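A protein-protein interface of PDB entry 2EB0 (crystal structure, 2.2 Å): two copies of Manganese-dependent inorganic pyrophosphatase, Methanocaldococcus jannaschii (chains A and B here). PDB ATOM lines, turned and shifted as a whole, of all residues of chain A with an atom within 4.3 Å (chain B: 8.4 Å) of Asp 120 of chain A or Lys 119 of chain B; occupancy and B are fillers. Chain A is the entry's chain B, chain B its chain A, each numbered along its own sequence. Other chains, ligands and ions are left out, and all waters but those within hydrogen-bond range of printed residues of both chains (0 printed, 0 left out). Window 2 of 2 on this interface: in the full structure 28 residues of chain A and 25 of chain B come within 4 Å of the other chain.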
ATOM      1  N   LEU A 116      -6.014 -29.260  29.585  1.00  0.00           N
ATOM      2  CA  LEU A 116      -5.257 -28.021  29.613  1.00  0.00           C
ATOM      3  C   LEU A 116      -3.814 -28.346  29.954  1.00  0.00           C
ATOM      4  O   LEU A 116      -2.871 -27.760  29.403  1.00  0.00           O
ATOM      5  CB  LEU A 116      -5.816 -27.064  30.659  1.00  0.00           C
ATOM      6  CG  LEU A 116      -7.139 -26.402  30.289  1.00  0.00           C
ATOM      7  CD1 LEU A 116      -7.513 -25.405  31.378  1.00  0.00           C
ATOM      8  CD2 LEU A 116      -6.990 -25.688  28.938  1.00  0.00           C
ATOM      9  N   TYR A 117      -3.646 -29.298  30.865  1.00  0.00           N
ATOM     10  CA  TYR A 117      -2.312 -29.675  31.283  1.00  0.00           C
ATOM     11  C   TYR A 117      -1.443 -30.236  30.170  1.00  0.00           C
ATOM     12  O   TYR A 117      -0.344 -29.741  29.934  1.00  0.00           O
ATOM     13  CB  TYR A 117      -2.371 -30.682  32.422  1.00  0.00           C
ATOM     14  CG  TYR A 117      -1.018 -31.218  32.775  1.00  0.00           C
ATOM     15  CD1 TYR A 117      -0.624 -32.489  32.363  1.00  0.00           C
ATOM     16  CD2 TYR A 117      -0.111 -30.439  33.483  1.00  0.00           C
ATOM     17  CE1 TYR A 117       0.643 -32.971  32.646  1.00  0.00           C
ATOM     18  CE2 TYR A 117       1.157 -30.904  33.770  1.00  0.00           C
ATOM     19  CZ  TYR A 117       1.530 -32.170  33.351  1.00  0.00           C
ATOM     20  OH  TYR A 117       2.786 -32.635  33.634  1.00  0.00           O
ATOM     21  N   PHE A 118      -1.929 -31.265  29.491  1.00  0.00           N
ATOM     22  CA  PHE A 118      -1.151 -31.882  28.433  1.00  0.00           C
ATOM     23  C   PHE A 118      -0.913 -30.982  27.228  1.00  0.00           C
ATOM     24  O   PHE A 118       0.077 -31.149  26.514  1.00  0.00           O
ATOM     25  CB  PHE A 118      -1.793 -33.199  28.016  1.00  0.00           C
ATOM     26  CG  PHE A 118      -1.694 -34.270  29.067  1.00  0.00           C
ATOM     27  CD1 PHE A 118      -2.841 -34.786  29.672  1.00  0.00           C
ATOM     28  CD2 PHE A 118      -0.445 -34.766  29.455  1.00  0.00           C
ATOM     29  CE1 PHE A 118      -2.749 -35.784  30.649  1.00  0.00           C
ATOM     30  CE2 PHE A 118      -0.340 -35.756  30.425  1.00  0.00           C
ATOM     31  CZ  PHE A 118      -1.498 -36.271  31.027  1.00  0.00           C
ATOM     32  N   LYS A 119      -1.808 -30.027  26.997  1.00  0.00           N
ATOM     33  CA  LYS A 119      -1.616 -29.100  25.885  1.00  0.00           C
ATOM     34  C   LYS A 119      -0.635 -27.997  26.300  1.00  0.00           C
ATOM     35  O   LYS A 119      -0.367 -27.082  25.532  1.00  0.00           O
ATOM     36  CB  LYS A 119      -2.946 -28.472  25.463  1.00  0.00           C
ATOM     37  CG  LYS A 119      -3.904 -29.445  24.803  1.00  0.00           C
ATOM     38  CD  LYS A 119      -5.212 -28.773  24.429  1.00  0.00           C
ATOM     39  CE  LYS A 119      -4.994 -27.684  23.401  1.00  0.00           C
ATOM     40  NZ  LYS A 119      -4.436 -28.250  22.152  1.00  0.00           N
ATOM     41  N   ASP A 120      -0.100 -28.096  27.516  1.00  0.00           N
ATOM     42  CA  ASP A 120       0.835 -27.094  28.019  1.00  0.00           C
ATOM     43  C   ASP A 120       0.179 -25.717  28.058  1.00  0.00           C
ATOM     44  O   ASP A 120       0.829 -24.703  27.796  1.00  0.00           O
ATOM     45  CB  ASP A 120       2.083 -27.034  27.133  1.00  0.00           C
ATOM     46  CG  ASP A 120       3.043 -28.167  27.406  1.00  0.00           C
ATOM     47  OD1 ASP A 120       3.676 -28.155  28.482  1.00  0.00           O
ATOM     48  OD2 ASP A 120       3.159 -29.069  26.550  1.00  0.00           O
ATOM     49  N   ALA A 121      -1.105 -25.687  28.395  1.00  0.00           N
ATOM     50  CA  ALA A 121      -1.837 -24.431  28.442  1.00  0.00           C
ATOM     51  C   ALA A 121      -2.561 -24.218  29.764  1.00  0.00           C
ATOM     52  O   ALA A 121      -3.590 -23.545  29.814  1.00  0.00           O
ATOM     53  CB  ALA A 121      -2.828 -24.376  27.297  1.00  0.00           C
ATOM     54  N   ILE A 122      -2.017 -24.775  30.838  1.00  0.00           N
ATOM     55  CA  ILE A 122      -2.637 -24.630  32.144  1.00  0.00           C
ATOM     56  C   ILE A 122      -2.617 -23.149  32.559  1.00  0.00           C
ATOM     57  O   ILE A 122      -3.454 -22.692  33.348  1.00  0.00           O
ATOM     58  CB  ILE A 122      -1.901 -25.509  33.190  1.00  0.00           C
ATOM     59  CG1 ILE A 122      -2.910 -26.120  34.168  1.00  0.00           C
ATOM     60  CG2 ILE A 122      -0.836 -24.700  33.909  1.00  0.00           C
ATOM     61  CD1 ILE A 122      -3.790 -25.122  34.876  1.00  0.00           C
ATOM     62  N   ASP A 123      -1.672 -22.399  31.998  1.00  0.00           N
ATOM     63  CA  ASP A 123      -1.537 -20.979  32.303  1.00  0.00           C
ATOM     64  C   ASP A 123      -2.712 -20.166  31.766  1.00  0.00           C
ATOM     65  O   ASP A 123      -2.884 -19.003  32.120  1.00  0.00           O
ATOM     66  CB  ASP A 123      -0.214 -20.448  31.744  1.00  0.00           C
ATOM     67  CG  ASP A 123      -0.067 -20.689  30.255  1.00  0.00           C
ATOM     68  OD1 ASP A 123      -0.421 -21.792  29.788  1.00  0.00           O
ATOM     69  OD2 ASP A 123       0.418 -19.776  29.553  1.00  0.00           O
ATOM     70  N   LYS A 129       2.452 -23.758  35.250  1.00  0.00           N
ATOM     71  CA  LYS A 129       3.276 -24.713  34.508  1.00  0.00           C
ATOM     72  C   LYS A 129       4.045 -25.731  35.346  1.00  0.00           C
ATOM     73  O   LYS A 129       5.147 -26.146  34.979  1.00  0.00           O
ATOM     74  CB  LYS A 129       4.259 -23.962  33.601  1.00  0.00           C
ATOM     75  CG  LYS A 129       3.595 -23.187  32.470  1.00  0.00           C
ATOM     76  CD  LYS A 129       3.018 -24.121  31.409  1.00  0.00           C
ATOM     77  CE  LYS A 129       2.164 -23.360  30.400  1.00  0.00           C
ATOM     78  NZ  LYS A 129       2.901 -22.238  29.747  1.00  0.00           N
ATOM     79  N   TYR B 102     -16.610 -20.248  27.668  1.00  0.00           N
ATOM     80  CA  TYR B 102     -15.282 -19.706  27.871  1.00  0.00           C
ATOM     81  C   TYR B 102     -15.352 -18.195  27.846  1.00  0.00           C
ATOM     82  O   TYR B 102     -15.626 -17.585  26.806  1.00  0.00           O
ATOM     83  CB  TYR B 102     -14.319 -20.199  26.794  1.00  0.00           C
ATOM     84  CG  TYR B 102     -12.894 -19.755  27.023  1.00  0.00           C
ATOM     85  CD1 TYR B 102     -12.331 -19.784  28.302  1.00  0.00           C
ATOM     86  CD2 TYR B 102     -12.095 -19.339  25.964  1.00  0.00           C
ATOM     87  CE1 TYR B 102     -11.008 -19.412  28.512  1.00  0.00           C
ATOM     88  CE2 TYR B 102     -10.765 -18.968  26.163  1.00  0.00           C
ATOM     89  CZ  TYR B 102     -10.230 -19.007  27.435  1.00  0.00           C
ATOM     90  OH  TYR B 102      -8.915 -18.659  27.637  1.00  0.00           O
ATOM     91  N   VAL B 112      -9.960 -12.853  23.340  1.00  0.00           N
ATOM     92  CA  VAL B 112     -10.081 -14.216  23.845  1.00  0.00           C
ATOM     93  C   VAL B 112      -9.801 -15.245  22.756  1.00  0.00           C
ATOM     94  O   VAL B 112      -9.064 -16.208  22.970  1.00  0.00           O
ATOM     95  CB  VAL B 112     -11.492 -14.477  24.400  1.00  0.00           C
ATOM     96  CG1 VAL B 112     -11.616 -15.934  24.827  1.00  0.00           C
ATOM     97  CG2 VAL B 112     -11.776 -13.534  25.564  1.00  0.00           C
ATOM     98  N   ILE B 113     -10.404 -15.032  21.591  1.00  0.00           N
ATOM     99  CA  ILE B 113     -10.235 -15.926  20.451  1.00  0.00           C
ATOM    100  C   ILE B 113      -8.764 -15.946  20.039  1.00  0.00           C
ATOM    101  O   ILE B 113      -8.158 -17.008  19.867  1.00  0.00           O
ATOM    102  CB  ILE B 113     -11.041 -15.441  19.224  1.00  0.00           C
ATOM    103  CG1 ILE B 113     -12.532 -15.294  19.568  1.00  0.00           C
ATOM    104  CG2 ILE B 113     -10.812 -16.393  18.057  1.00  0.00           C
ATOM    105  CD1 ILE B 113     -13.270 -16.580  19.725  1.00  0.00           C
ATOM    106  N   ALA B 114      -8.206 -14.753  19.871  1.00  0.00           N
ATOM    107  CA  ALA B 114      -6.822 -14.600  19.461  1.00  0.00           C
ATOM    108  C   ALA B 114      -5.840 -15.306  20.395  1.00  0.00           C
ATOM    109  O   ALA B 114      -4.910 -15.969  19.920  1.00  0.00           O
ATOM    110  CB  ALA B 114      -6.486 -13.121  19.349  1.00  0.00           C
ATOM    111  N   GLU B 115      -6.041 -15.175  21.709  1.00  0.00           N
ATOM    112  CA  GLU B 115      -5.146 -15.816  22.671  1.00  0.00           C
ATOM    113  C   GLU B 115      -5.204 -17.331  22.559  1.00  0.00           C
ATOM    114  O   GLU B 115      -4.202 -18.014  22.759  1.00  0.00           O
ATOM    115  CB  GLU B 115      -5.472 -15.417  24.114  1.00  0.00           C
ATOM    116  CG  GLU B 115      -4.484 -16.026  25.109  1.00  0.00           C
ATOM    117  CD  GLU B 115      -4.851 -15.807  26.571  1.00  0.00           C
ATOM    118  OE1 GLU B 115      -5.969 -16.195  26.979  1.00  0.00           O
ATOM    119  OE2 GLU B 115      -4.010 -15.260  27.316  1.00  0.00           O
ATOM    120  N   LEU B 116      -6.379 -17.863  22.254  1.00  0.00           N
ATOM    121  CA  LEU B 116      -6.507 -19.297  22.101  1.00  0.00           C
ATOM    122  C   LEU B 116      -5.762 -19.713  20.840  1.00  0.00           C
ATOM    123  O   LEU B 116      -5.094 -20.751  20.813  1.00  0.00           O
ATOM    124  CB  LEU B 116      -7.976 -19.706  21.991  1.00  0.00           C
ATOM    125  CG  LEU B 116      -8.780 -19.767  23.290  1.00  0.00           C
ATOM    126  CD1 LEU B 116     -10.168 -20.262  22.963  1.00  0.00           C
ATOM    127  CD2 LEU B 116      -8.096 -20.681  24.318  1.00  0.00           C
ATOM    128  N   TYR B 117      -5.860 -18.891  19.798  1.00  0.00           N
ATOM    129  CA  TYR B 117      -5.192 -19.213  18.547  1.00  0.00           C
ATOM    130  C   TYR B 117      -3.671 -19.252  18.640  1.00  0.00           C
ATOM    131  O   TYR B 117      -3.054 -20.242  18.250  1.00  0.00           O
ATOM    132  CB  TYR B 117      -5.593 -18.240  17.439  1.00  0.00           C
ATOM    133  CG  TYR B 117      -4.810 -18.475  16.172  1.00  0.00           C
ATOM    134  CD1 TYR B 117      -3.673 -17.717  15.875  1.00  0.00           C
ATOM    135  CD2 TYR B 117      -5.180 -19.486  15.281  1.00  0.00           C
ATOM    136  CE1 TYR B 117      -2.925 -17.961  14.718  1.00  0.00           C
ATOM    137  CE2 TYR B 117      -4.445 -19.735  14.131  1.00  0.00           C
ATOM    138  CZ  TYR B 117      -3.320 -18.968  13.853  1.00  0.00           C
ATOM    139  OH  TYR B 117      -2.615 -19.201  12.698  1.00  0.00           O
ATOM    140  N   PHE B 118      -3.071 -18.176  19.141  1.00  0.00           N
ATOM    141  CA  PHE B 118      -1.620 -18.112  19.257  1.00  0.00           C
ATOM    142  C   PHE B 118      -1.075 -19.141  20.240  1.00  0.00           C
ATOM    143  O   PHE B 118       0.041 -19.631  20.080  1.00  0.00           O
ATOM    144  CB  PHE B 118      -1.182 -16.703  19.673  1.00  0.00           C
ATOM    145  CG  PHE B 118      -1.407 -15.658  18.608  1.00  0.00           C
ATOM    146  CD1 PHE B 118      -2.277 -14.597  18.825  1.00  0.00           C
ATOM    147  CD2 PHE B 118      -0.772 -15.757  17.374  1.00  0.00           C
ATOM    148  CE1 PHE B 118      -2.518 -13.646  17.829  1.00  0.00           C
ATOM    149  CE2 PHE B 118      -1.004 -14.816  16.368  1.00  0.00           C
ATOM    150  CZ  PHE B 118      -1.882 -13.757  16.597  1.00  0.00           C
ATOM    151  N   LYS B 119      -1.874 -19.473  21.247  1.00  0.00           N
ATOM    152  CA  LYS B 119      -1.477 -20.440  22.263  1.00  0.00           C
ATOM    153  C   LYS B 119      -1.648 -21.867  21.746  1.00  0.00           C
ATOM    154  O   LYS B 119      -1.414 -22.826  22.477  1.00  0.00           O
ATOM    155  CB  LYS B 119      -2.337 -20.246  23.517  1.00  0.00           C
ATOM    156  CG  LYS B 119      -1.858 -20.973  24.763  1.00  0.00           C
ATOM    157  CD  LYS B 119      -0.637 -20.294  25.358  1.00  0.00           C
ATOM    158  CE  LYS B 119      -0.297 -20.863  26.724  1.00  0.00           C
ATOM    159  NZ  LYS B 119      -0.042 -22.325  26.668  1.00  0.00           N
ATOM    160  N   ASP B 120      -2.057 -21.999  20.487  1.00  0.00           N
ATOM    161  CA  ASP B 120      -2.286 -23.307  19.874  1.00  0.00           C
ATOM    162  C   ASP B 120      -3.398 -24.057  20.609  1.00  0.00           C
ATOM    163  O   ASP B 120      -3.412 -25.295  20.651  1.00  0.00           O
ATOM    164  CB  ASP B 120      -1.005 -24.145  19.895  1.00  0.00           C
ATOM    165  CG  ASP B 120       0.123 -23.508  19.115  1.00  0.00           C
ATOM    166  OD1 ASP B 120      -0.057 -23.254  17.904  1.00  0.00           O
ATOM    167  OD2 ASP B 120       1.192 -23.259  19.710  1.00  0.00           O
ATOM    168  N   ALA B 121      -4.344 -23.311  21.175  1.00  0.00           N
ATOM    169  CA  ALA B 121      -5.432 -23.932  21.917  1.00  0.00           C
ATOM    170  C   ALA B 121      -6.819 -23.708  21.322  1.00  0.00           C
ATOM    171  O   ALA B 121      -7.824 -23.861  22.014  1.00  0.00           O
ATOM    172  CB  ALA B 121      -5.400 -23.459  23.371  1.00  0.00           C
ATOM    173  N   ILE B 122      -6.881 -23.355  20.042  1.00  0.00           N
ATOM    174  CA  ILE B 122      -8.172 -23.148  19.391  1.00  0.00           C
ATOM    175  C   ILE B 122      -9.046 -24.395  19.499  1.00  0.00           C
ATOM    176  O   ILE B 122     -10.270 -24.304  19.623  1.00  0.00           O
ATOM    177  CB  ILE B 122      -8.033 -22.791  17.887  1.00  0.00           C
ATOM    178  CG1 ILE B 122      -6.700 -23.304  17.325  1.00  0.00           C
ATOM    179  CG2 ILE B 122      -8.207 -21.296  17.702  1.00  0.00           C
ATOM    180  CD1 ILE B 122      -5.461 -22.514  17.762  1.00  0.00           C
ATOM    181  N   ASP B 123      -8.415 -25.560  19.451  1.00  0.00           N
ATOM    182  CA  ASP B 123      -9.151 -26.812  19.544  1.00  0.00           C
ATOM    183  C   ASP B 123      -9.899 -26.954  20.871  1.00  0.00           C
ATOM    184  O   ASP B 123     -10.815 -27.763  20.976  1.00  0.00           O
ATOM    185  CB  ASP B 123      -8.192 -27.986  19.359  1.00  0.00           C
ATOM    186  CG  ASP B 123      -7.005 -27.909  20.287  1.00  0.00           C
ATOM    187  OD1 ASP B 123      -6.311 -26.871  20.276  1.00  0.00           O
ATOM    188  OD2 ASP B 123      -6.764 -28.881  21.029  1.00  0.00           O
ATOM    189  N   LEU B 124      -9.512 -26.172  21.876  1.00  0.00           N
ATOM    190  CA  LEU B 124     -10.161 -26.234  23.184  1.00  0.00           C
ATOM    191  C   LEU B 124     -11.629 -25.816  23.136  1.00  0.00           C
ATOM    192  O   LEU B 124     -12.402 -26.149  24.037  1.00  0.00           O
ATOM    193  CB  LEU B 124      -9.426 -25.356  24.207  1.00  0.00           C
ATOM    194  CG  LEU B 124      -8.078 -25.839  24.768  1.00  0.00           C
ATOM    195  CD1 LEU B 124      -7.502 -24.781  25.702  1.00  0.00           C
ATOM    196  CD2 LEU B 124      -8.265 -27.164  25.505  1.00  0.00           C
ATOM    197  N   GLU B 162      -1.172  -6.836  23.777  1.00  0.00           N
ATOM    198  CA  GLU B 162      -0.294  -7.911  23.322  1.00  0.00           C
ATOM    199  C   GLU B 162      -0.900  -8.685  22.157  1.00  0.00           C
ATOM    200  O   GLU B 162      -0.187  -9.150  21.270  1.00  0.00           O
ATOM    201  CB  GLU B 162      -0.016  -8.875  24.474  1.00  0.00           C
ATOM    202  CG  GLU B 162       0.930 -10.010  24.137  1.00  0.00           C
ATOM    203  CD  GLU B 162       1.034 -11.021  25.266  1.00  0.00           C
ATOM    204  OE1 GLU B 162       1.185 -10.594  26.432  1.00  0.00           O
ATOM    205  OE2 GLU B 162       0.969 -12.238  24.991  1.00  0.00           O
ATOM    206  N   MET B 163      -2.218  -8.834  22.158  1.00  0.00           N
ATOM    207  CA  MET B 163      -2.857  -9.568  21.079  1.00  0.00           C
ATOM    208  C   MET B 163      -2.976  -8.686  19.844  1.00  0.00           C
ATOM    209  O   MET B 163      -2.803  -9.159  18.721  1.00  0.00           O
ATOM    210  CB  MET B 163      -4.231 -10.076  21.517  1.00  0.00           C
ATOM    211  CG  MET B 163      -4.465 -11.539  21.169  1.00  0.00           C
ATOM    212  SD  MET B 163      -3.517 -12.744  22.139  1.00  0.00           S
ATOM    213  CE  MET B 163      -1.871 -12.545  21.531  1.00  0.00           C
ATOM    214  N   LYS B 166       0.247  -8.787  17.905  1.00  0.00           N
ATOM    215  CA  LYS B 166       0.405 -10.012  17.131  1.00  0.00           C
ATOM    216  C   LYS B 166      -0.498 -10.085  15.901  1.00  0.00           C
ATOM    217  O   LYS B 166      -0.063 -10.497  14.821  1.00  0.00           O
ATOM    218  CB  LYS B 166       0.150 -11.227  18.019  1.00  0.00           C
ATOM    219  CG  LYS B 166       1.218 -11.461  19.069  1.00  0.00           C
ATOM    220  CD  LYS B 166       1.068 -12.841  19.675  1.00  0.00           C
ATOM    221  CE  LYS B 166       2.239 -13.174  20.576  1.00  0.00           C
ATOM    222  NZ  LYS B 166       2.227 -14.609  20.965  1.00  0.00           N
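The backbone carbonyl oxygen of Asp 120 of chain B sits at hydrogen-bond distance from the side-chain amino group of Lys 119 of chain A, at 3.5 Å. The side-chain carboxylate (OD2) of Asp 123 of chain B is in salt-bridge range of the side-chain amino group (NZ) of Lys 119 of chain A. The backbone carbonyl oxygen of Asp 120 of chain A lies within hydrogen-bond range of the side-chain amino group of Lys 119 of chain B. The side-chain amino group (NZ) of Lys 119 of chain B lies within salt-bridge range of the side-chain carboxylate (OD1) of Asp 123 of chain A (3.2 Å).
N of Ile 122 of chain A sits at hydrogen-bond distance from O of Leu 116 of chain A (3.4 Å). The side-chain carboxylate (OD1) of Asp 123 of chain A lies within salt-bridge range of the side-chain amino group (NZ) of Lys 129 of chain A (3.4 Å). N of Ala 121 of chain A lies within hydrogen-bond range of O of Leu 116 of chain A (2.9 Å).
Among the printed residues, pairs that only touch across the chains: Leu 116 of chain A with Leu 124 of chain B (3.4 Å), Lys 119 of chain A with Leu 124 of chain B (3.6 Å) and Ala 121 of chain A with Lys 119 of chain B (3.3 Å).
Phe 118 of chain A touches none of the printed residues of chain B. Printed residues of chain B within 4 Å of Lys 119 of chain A: Asp 120 (3.5 Å), Asp 123 (2.7 Å) and Leu 124 (3.6 Å). Of chain B, only Lys 119 (2.8 Å) comes within 4 Å of Asp 120 of chain A. Of the printed residues of chain B, Ala 121 of chain A touches Lys 119 (3.3 Å). Of the printed residues of chain B, Asp 123 of chain A touches Lys 119 (3.1 Å). Tyr 117 of chain B touches none of the printed residues of chain A. Lys 119 of chain B touches just these residues of chain A: Asp 120 (2.8 Å), Ala 121 (3.3 Å) and Asp 123 (3.1 Å). Of the printed residues of chain A, Asp 120 of chain B touches Lys 119 (3.5 Å). Of the printed residues of chain A, Leu 124 of chain B touches Leu 116 and Lys 119. The nearest printed residue of chain A that does not touch Lys 119 of chain B is Lys 129 of chain A (4.3 Å).
Of the 9 printed residues of chain A, 5 touch a printed residue of chain B. Among the printed residues, Asp or Glu carboxylates within 4 Å of a Lys or Arg side-chain nitrogen of the other chain: Lys 119 of chain A with Asp 123 of chain B and Asp 123 of chain A with Lys 119 of chain B.
Lys 119 of chain A touches Asp 120 of chain B, and with the chains exchanged Asp 120 of chain A touches Lys 119 of chain B. Lys 119 of chain A touches Asp 123 of chain B, and with the chains exchanged Asp 123 of chain A touches Lys 119 of chain B. Ala 121 of chain A touches Lys 119 of chain B, but with the chains exchanged Lys 119 of chain A does not touch Ala 121 of chain B (4.1 Å). Positions printed for both chains: 116, 117, 118, 119, 120, 121, 122 and 123.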
